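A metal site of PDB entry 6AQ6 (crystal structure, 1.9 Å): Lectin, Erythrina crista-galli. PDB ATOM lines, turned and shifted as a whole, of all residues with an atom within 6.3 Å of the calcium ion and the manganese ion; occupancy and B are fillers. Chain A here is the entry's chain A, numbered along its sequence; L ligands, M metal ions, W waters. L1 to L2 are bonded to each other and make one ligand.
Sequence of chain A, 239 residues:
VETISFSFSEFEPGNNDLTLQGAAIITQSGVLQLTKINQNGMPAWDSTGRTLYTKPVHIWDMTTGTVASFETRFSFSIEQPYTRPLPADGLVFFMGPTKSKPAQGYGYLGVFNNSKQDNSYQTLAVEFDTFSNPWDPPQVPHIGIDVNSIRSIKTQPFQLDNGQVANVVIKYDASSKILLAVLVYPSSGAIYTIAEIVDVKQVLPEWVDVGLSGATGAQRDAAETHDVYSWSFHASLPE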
ATOM      1  N   ASP A  89       6.431  -9.483   2.061  1.00  0.00           N
ATOM      2  CA  ASP A  89       7.307  -9.130   0.936  1.00  0.00           C
ATOM      3  C   ASP A  89       6.775  -7.914   0.156  1.00  0.00           C
ATOM      4  O   ASP A  89       7.532  -7.194  -0.476  1.00  0.00           O
ATOM      5  CB  ASP A  89       7.442 -10.308  -0.061  1.00  0.00           C
ATOM      6  CG  ASP A  89       8.647 -11.222   0.240  1.00  0.00           C
ATOM      7  OD1 ASP A  89       8.406 -12.300   0.804  1.00  0.00           O
ATOM      8  OD2 ASP A  89       9.796 -10.849  -0.073  1.00  0.00           O
ATOM      9  N   GLY A 107       9.290 -12.857  -2.651  1.00  0.00           N
ATOM     10  CA  GLY A 107       9.797 -11.713  -3.373  1.00  0.00           C
ATOM     11  C   GLY A 107       9.299 -11.627  -4.805  1.00  0.00           C
ATOM     12  O   GLY A 107       9.571 -10.613  -5.464  1.00  0.00           O
ATOM     13  N   LEU A 109       6.052 -11.790  -5.359  1.00  0.00           N
ATOM     14  CA  LEU A 109       4.870 -10.959  -5.145  1.00  0.00           C
ATOM     15  C   LEU A 109       3.603 -11.535  -5.742  1.00  0.00           C
ATOM     16  O   LEU A 109       2.597 -10.817  -5.869  1.00  0.00           O
ATOM     17  CB  LEU A 109       5.109  -9.539  -5.685  1.00  0.00           C
ATOM     18  CG  LEU A 109       6.288  -8.788  -5.074  1.00  0.00           C
ATOM     19  CD1 LEU A 109       6.375  -7.331  -5.573  1.00  0.00           C
ATOM     20  CD2 LEU A 109       6.216  -8.832  -3.537  1.00  0.00           C
ATOM     21  N   GLU A 127       5.203  -1.841  -8.190  1.00  0.00           N
ATOM     22  CA  GLU A 127       5.328  -2.633  -6.977  1.00  0.00           C
ATOM     23  C   GLU A 127       5.620  -1.707  -5.798  1.00  0.00           C
ATOM     24  O   GLU A 127       6.218  -0.637  -5.963  1.00  0.00           O
ATOM     25  CB  GLU A 127       6.445  -3.670  -7.104  1.00  0.00           C
ATOM     26  CG  GLU A 127       7.837  -3.059  -7.169  1.00  0.00           C
ATOM     27  CD  GLU A 127       8.967  -4.078  -7.039  1.00  0.00           C
ATOM     28  OE1 GLU A 127       8.851  -5.198  -7.596  1.00  0.00           O
ATOM     29  OE2 GLU A 127       9.974  -3.770  -6.386  1.00  0.00           O
ATOM     30  N   ASP A 129       7.498  -2.594  -2.517  1.00  0.00           N
ATOM     31  CA  ASP A 129       8.325  -3.749  -2.180  1.00  0.00           C
ATOM     32  C   ASP A 129       8.915  -3.512  -0.800  1.00  0.00           C
ATOM     33  O   ASP A 129       9.567  -2.485  -0.587  1.00  0.00           O
ATOM     34  CB  ASP A 129       9.415  -3.873  -3.250  1.00  0.00           C
ATOM     35  CG  ASP A 129      10.191  -5.179  -3.185  1.00  0.00           C
ATOM     36  OD1 ASP A 129      10.165  -5.794  -2.107  1.00  0.00           O
ATOM     37  OD2 ASP A 129      10.829  -5.578  -4.228  1.00  0.00           O
ATOM     38  N   THR A 130       8.685  -4.441   0.137  1.00  0.00           N
ATOM     39  CA  THR A 130       9.065  -4.266   1.535  1.00  0.00           C
ATOM     40  C   THR A 130      10.259  -5.104   1.987  1.00  0.00           C
ATOM     41  O   THR A 130      10.686  -4.960   3.140  1.00  0.00           O
ATOM     42  CB  THR A 130       7.873  -4.584   2.450  1.00  0.00           C
ATOM     43  OG1 THR A 130       7.402  -5.912   2.190  1.00  0.00           O
ATOM     44  CG2 THR A 130       6.739  -3.567   2.246  1.00  0.00           C
ATOM     45  N   PHE A 131      10.802  -5.978   1.132  1.00  0.00           N
ATOM     46  CA  PHE A 131      11.939  -6.821   1.514  1.00  0.00           C
ATOM     47  C   PHE A 131      12.980  -6.798   0.401  1.00  0.00           C
ATOM     48  O   PHE A 131      12.639  -6.990  -0.770  1.00  0.00           O
ATOM     49  CB  PHE A 131      11.476  -8.259   1.803  1.00  0.00           C
ATOM     50  CG  PHE A 131      12.602  -9.205   2.139  1.00  0.00           C
ATOM     51  CD1 PHE A 131      13.022  -9.361   3.443  1.00  0.00           C
ATOM     52  CD2 PHE A 131      13.226  -9.949   1.144  1.00  0.00           C
ATOM     53  CE1 PHE A 131      14.068 -10.223   3.769  1.00  0.00           C
ATOM     54  CE2 PHE A 131      14.268 -10.827   1.455  1.00  0.00           C
ATOM     55  CZ  PHE A 131      14.689 -10.958   2.771  1.00  0.00           C
ATOM     56  N   SER A 132      14.240  -6.579   0.759  1.00  0.00           N
ATOM     57  CA  SER A 132      15.315  -6.422  -0.226  1.00  0.00           C
ATOM     58  C   SER A 132      15.905  -7.779  -0.620  1.00  0.00           C
ATOM     59  O   SER A 132      16.795  -8.305   0.056  1.00  0.00           O
ATOM     60  CB  SER A 132      16.397  -5.493   0.310  1.00  0.00           C
ATOM     61  OG  SER A 132      17.411  -5.250  -0.657  1.00  0.00           O
ATOM     62  N   ASN A 133      15.423  -8.329  -1.745  1.00  0.00           N
ATOM     63  CA  ASN A 133      15.929  -9.570  -2.325  1.00  0.00           C
ATOM     64  C   ASN A 133      17.260  -9.324  -3.031  1.00  0.00           C
ATOM     65  O   ASN A 133      17.672  -8.177  -3.204  1.00  0.00           O
ATOM     66  CB  ASN A 133      14.914 -10.140  -3.331  1.00  0.00           C
ATOM     67  CG  ASN A 133      13.596 -10.530  -2.684  1.00  0.00           C
ATOM     68  OD1 ASN A 133      12.652  -9.741  -2.634  1.00  0.00           O
ATOM     69  ND2 ASN A 133      13.507 -11.782  -2.220  1.00  0.00           N
ATOM     70  N   TRP A 135      17.878  -9.252  -6.106  1.00  0.00           N
ATOM     71  CA  TRP A 135      17.692  -8.462  -7.311  1.00  0.00           C
ATOM     72  C   TRP A 135      17.209  -7.040  -7.040  1.00  0.00           C
ATOM     73  O   TRP A 135      17.104  -6.258  -7.988  1.00  0.00           O
ATOM     74  CB  TRP A 135      16.670  -9.136  -8.230  1.00  0.00           C
ATOM     75  CG  TRP A 135      15.390  -9.500  -7.493  1.00  0.00           C
ATOM     76  CD1 TRP A 135      14.346  -8.672  -7.196  1.00  0.00           C
ATOM     77  CD2 TRP A 135      15.040 -10.793  -6.970  1.00  0.00           C
ATOM     78  NE1 TRP A 135      13.373  -9.362  -6.524  1.00  0.00           N
ATOM     79  CE2 TRP A 135      13.773 -10.666  -6.371  1.00  0.00           C
ATOM     80  CE3 TRP A 135      15.685 -12.026  -6.939  1.00  0.00           C
ATOM     81  CZ2 TRP A 135      13.130 -11.727  -5.752  1.00  0.00           C
ATOM     82  CZ3 TRP A 135      15.049 -13.089  -6.333  1.00  0.00           C
ATOM     83  CH2 TRP A 135      13.784 -12.945  -5.752  1.00  0.00           C
ATOM     84  N   ASP A 136      16.880  -6.712  -5.760  1.00  0.00           N
ATOM     85  CA  ASP A 136      16.336  -5.459  -5.250  1.00  0.00           C
ATOM     86  C   ASP A 136      17.448  -4.475  -4.910  1.00  0.00           C
ATOM     87  O   ASP A 136      18.566  -4.882  -4.569  1.00  0.00           O
ATOM     88  CB  ASP A 136      15.501  -5.730  -4.002  1.00  0.00           C
ATOM     89  CG  ASP A 136      14.127  -6.201  -4.341  1.00  0.00           C
ATOM     90  OD1 ASP A 136      13.668  -5.718  -5.393  1.00  0.00           O
ATOM     91  OD2 ASP A 136      13.532  -7.042  -3.610  1.00  0.00           O
ATOM     92  N   PRO A 137      17.190  -3.166  -4.995  1.00  0.00           N
ATOM     93  CA  PRO A 137      18.109  -2.206  -4.390  1.00  0.00           C
ATOM     94  C   PRO A 137      18.173  -2.452  -2.892  1.00  0.00           C
ATOM     95  O   PRO A 137      17.317  -3.189  -2.369  1.00  0.00           O
ATOM     96  CB  PRO A 137      17.471  -0.843  -4.706  1.00  0.00           C
ATOM     97  CG  PRO A 137      16.013  -1.144  -4.842  1.00  0.00           C
ATOM     98  CD  PRO A 137      15.961  -2.522  -5.484  1.00  0.00           C
ATOM     99  N   VAL A 140      14.553  -0.541   1.406  1.00  0.00           N
ATOM    100  CA  VAL A 140      13.136  -0.906   1.450  1.00  0.00           C
ATOM    101  C   VAL A 140      12.458  -0.014   2.482  1.00  0.00           C
ATOM    102  O   VAL A 140      13.083   0.374   3.483  1.00  0.00           O
ATOM    103  CB  VAL A 140      12.947  -2.392   1.767  1.00  0.00           C
ATOM    104  CG1 VAL A 140      13.248  -3.253   0.534  1.00  0.00           C
ATOM    105  CG2 VAL A 140      13.802  -2.798   2.973  1.00  0.00           C
ATOM    106  N   HIS A 142      10.390   0.333  -1.335  1.00  0.00           N
ATOM    107  CA  HIS A 142      10.636   1.121  -2.533  1.00  0.00           C
ATOM    108  C   HIS A 142       9.491   0.880  -3.516  1.00  0.00           C
ATOM    109  O   HIS A 142       8.907  -0.206  -3.560  1.00  0.00           O
ATOM    110  CB  HIS A 142      11.982   0.783  -3.185  1.00  0.00           C
ATOM    111  CG  HIS A 142      12.164  -0.681  -3.507  1.00  0.00           C
ATOM    112  ND1 HIS A 142      13.033  -1.486  -2.806  1.00  0.00           N
ATOM    113  CD2 HIS A 142      11.602  -1.467  -4.450  1.00  0.00           C
ATOM    114  CE1 HIS A 142      12.987  -2.708  -3.299  1.00  0.00           C
ATOM    115  NE2 HIS A 142      12.124  -2.727  -4.295  1.00  0.00           N
ATOM    116  N   GLY A 144       8.680   0.349  -7.385  1.00  0.00           N
ATOM    117  CA  GLY A 144       9.390  -0.113  -8.558  1.00  0.00           C
ATOM    118  C   GLY A 144       8.440  -0.213  -9.742  1.00  0.00           C
ATOM    119  O   GLY A 144       7.271  -0.592  -9.609  1.00  0.00           O
ATOM    120  N   ASP A 146       8.006  -2.399 -12.893  1.00  0.00           N
ATOM    121  CA  ASP A 146       8.430  -3.748 -13.297  1.00  0.00           C
ATOM    122  C   ASP A 146       7.908  -4.009 -14.710  1.00  0.00           C
ATOM    123  O   ASP A 146       6.692  -4.106 -14.917  1.00  0.00           O
ATOM    124  CB  ASP A 146       7.895  -4.807 -12.344  1.00  0.00           C
ATOM    125  CG  ASP A 146       8.366  -4.613 -10.890  1.00  0.00           C
ATOM    126  OD1 ASP A 146       9.254  -3.783 -10.647  1.00  0.00           O
ATOM    127  OD2 ASP A 146       7.825  -5.316 -10.005  1.00  0.00           O
ATOM    128  N   ILE A 150      10.499  -9.024 -12.201  1.00  0.00           N
ATOM    129  CA  ILE A 150      10.515  -8.501 -10.830  1.00  0.00           C
ATOM    130  C   ILE A 150      11.708  -7.593 -10.596  1.00  0.00           C
ATOM    131  O   ILE A 150      11.738  -6.848  -9.603  1.00  0.00           O
ATOM    132  CB  ILE A 150      10.492  -9.684  -9.846  1.00  0.00           C
ATOM    133  CG1 ILE A 150      10.189  -9.185  -8.416  1.00  0.00           C
ATOM    134  CG2 ILE A 150      11.829 -10.441  -9.922  1.00  0.00           C
ATOM    135  CD1 ILE A 150       8.721  -8.776  -8.200  1.00  0.00           C
ATOM    136  N   SER A 152      13.116  -4.395 -11.251  1.00  0.00           N
ATOM    137  CA  SER A 152      12.524  -3.158 -11.733  1.00  0.00           C
ATOM    138  C   SER A 152      13.494  -2.394 -12.622  1.00  0.00           C
ATOM    139  O   SER A 152      14.701  -2.303 -12.354  1.00  0.00           O
ATOM    140  CB  SER A 152      12.123  -2.280 -10.532  1.00  0.00           C
ATOM    141  OG  SER A 152      11.450  -3.085  -9.581  1.00  0.00           O
ATOM    142  N   THR A 155      13.482   2.295  -9.615  1.00  0.00           N
ATOM    143  CA  THR A 155      13.032   2.189  -8.233  1.00  0.00           C
ATOM    144  C   THR A 155      13.134   3.535  -7.526  1.00  0.00           C
ATOM    145  O   THR A 155      13.926   4.398  -7.901  1.00  0.00           O
ATOM    146  CB  THR A 155      13.836   1.139  -7.430  1.00  0.00           C
ATOM    147  OG1 THR A 155      15.213   1.525  -7.336  1.00  0.00           O
ATOM    148  CG2 THR A 155      13.737  -0.232  -8.083  1.00  0.00           C
HETATM  149  C1  LIG L   1      15.747 -19.494   3.308  1.00  0.00           C
HETATM  150  C2  LIG L   1      15.261 -18.505   4.347  1.00  0.00           C
HETATM  151  C3  LIG L   1      14.121 -17.730   3.714  1.00  0.00           C
HETATM  152  C4  LIG L   1      14.644 -17.008   2.483  1.00  0.00           C
HETATM  153  C5  LIG L   1      15.520 -17.878   1.597  1.00  0.00           C
HETATM  154  C6  LIG L   1      16.401 -16.995   0.754  1.00  0.00           C
HETATM  155  C7  LIG L   1      15.476 -18.997   6.739  1.00  0.00           C
HETATM  156  C8  LIG L   1      14.995 -19.732   7.963  1.00  0.00           C
HETATM  157  N1  LIG L   1      14.810 -19.202   5.491  1.00  0.00           N
HETATM  158  O1  LIG L   1      16.684 -20.392   3.858  1.00  0.00           O
HETATM  159  O2  LIG L   1      13.518 -16.809   4.635  1.00  0.00           O
HETATM  160  O3  LIG L   1      13.541 -16.567   1.714  1.00  0.00           O
HETATM  161  O4  LIG L   1      16.382 -18.733   2.318  1.00  0.00           O
HETATM  162  O5  LIG L   1      17.014 -17.795  -0.238  1.00  0.00           O
HETATM  163  O6  LIG L   1      16.411 -18.228   6.847  1.00  0.00           O
HETATM  164  C1  LG2 L   2      13.348 -15.188   1.661  1.00  0.00           C
HETATM  165  C2  LG2 L   2      12.377 -14.834   0.530  1.00  0.00           C
HETATM  166  C3  LG2 L   2      12.097 -13.348   0.584  1.00  0.00           C
HETATM  167  C4  LG2 L   2      11.473 -13.047   1.928  1.00  0.00           C
HETATM  168  C5  LG2 L   2      12.394 -13.502   3.056  1.00  0.00           C
HETATM  169  C6  LG2 L   2      11.697 -13.350   4.401  1.00  0.00           C
HETATM  170  O1  LG2 L   2      12.930 -15.130  -0.739  1.00  0.00           O
HETATM  171  O2  LG2 L   2      11.300 -12.939  -0.518  1.00  0.00           O
HETATM  172  O3  LG2 L   2      10.261 -13.746   2.007  1.00  0.00           O
HETATM  173  O4  LG2 L   2      12.787 -14.851   2.928  1.00  0.00           O
HETATM  174  O5  LG2 L   2      12.496 -13.883   5.450  1.00  0.00           O
HETATM  175 CA    CA M   1      11.616  -7.578  -2.777  1.00  0.00          CA
HETATM  176 MN    MN M   2      11.793  -4.549  -5.684  1.00  0.00          MN
HETATM  177  O   HOH W   1      10.929  -6.403  -7.139  1.00  0.00           O
HETATM  178  O   HOH W   2      10.002  -8.698  -1.684  1.00  0.00           O
HETATM  179  O   HOH W   3      12.833  -3.763  -7.580  1.00  0.00           O
HETATM  180  O   HOH W   4      10.812  -8.483  -5.092  1.00  0.00           O
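O2 of LG2 L2 sits at hydrogen-bond distance from ND2 of Asn 133, 3.0 Å away.
O2 of LG2 L2 sits at hydrogen-bond distance from N of Gly 107, 2.9 Å away.
The side-chain carboxylate (OD2) of Asp 89 is in hydrogen-bond range of an oxygen (O2) of LG2 L2 (2.6 Å).
OE1 of Glu 127 lies close to OD2 of Asp 146, 2.6 Å away.
The backbone carbonyl oxygen (O) of Gly 144 lies within hydrogen-bond range of the backbone NH (N) of Glu 127, at 2.8 Å.
Of the 19 residues printed, 4 come within 4 Å of the calcium ion.
Within 4 Å of the manganese ion: Glu 127, Asp 129, Asp 136 and His 142.
The calcium ion is bound by OD2 of Asp 136, water W2, O of Phe 131, OD1 of Asp 129, OD1 of Asn 133, OD2 of Asp 129 and water W4.
The calcium ion has seven donor atoms within binding distance.
The manganese ion is bound by OD2 of Asp 129 (2.0 Å), OE2 of Glu 127 (2.1 Å), OD1 of Asp 136 (2.2 Å), water W3 (2.3 Å), NE2 of His 142 (2.3 Å) and water W1 (2.5 Å).
The manganese ion has six donor atoms within binding distance.
Water W4 lies within hydrogen-bond range of the backbone carbonyl oxygen (O) of Gly 107 (2.5 Å) and the indole nitrogen (NE1) of Trp 135 (3.1 Å).
Water W1 bridges the side-chain carboxylate of Glu 127 and the backbone carbonyl oxygen of Ile 150.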
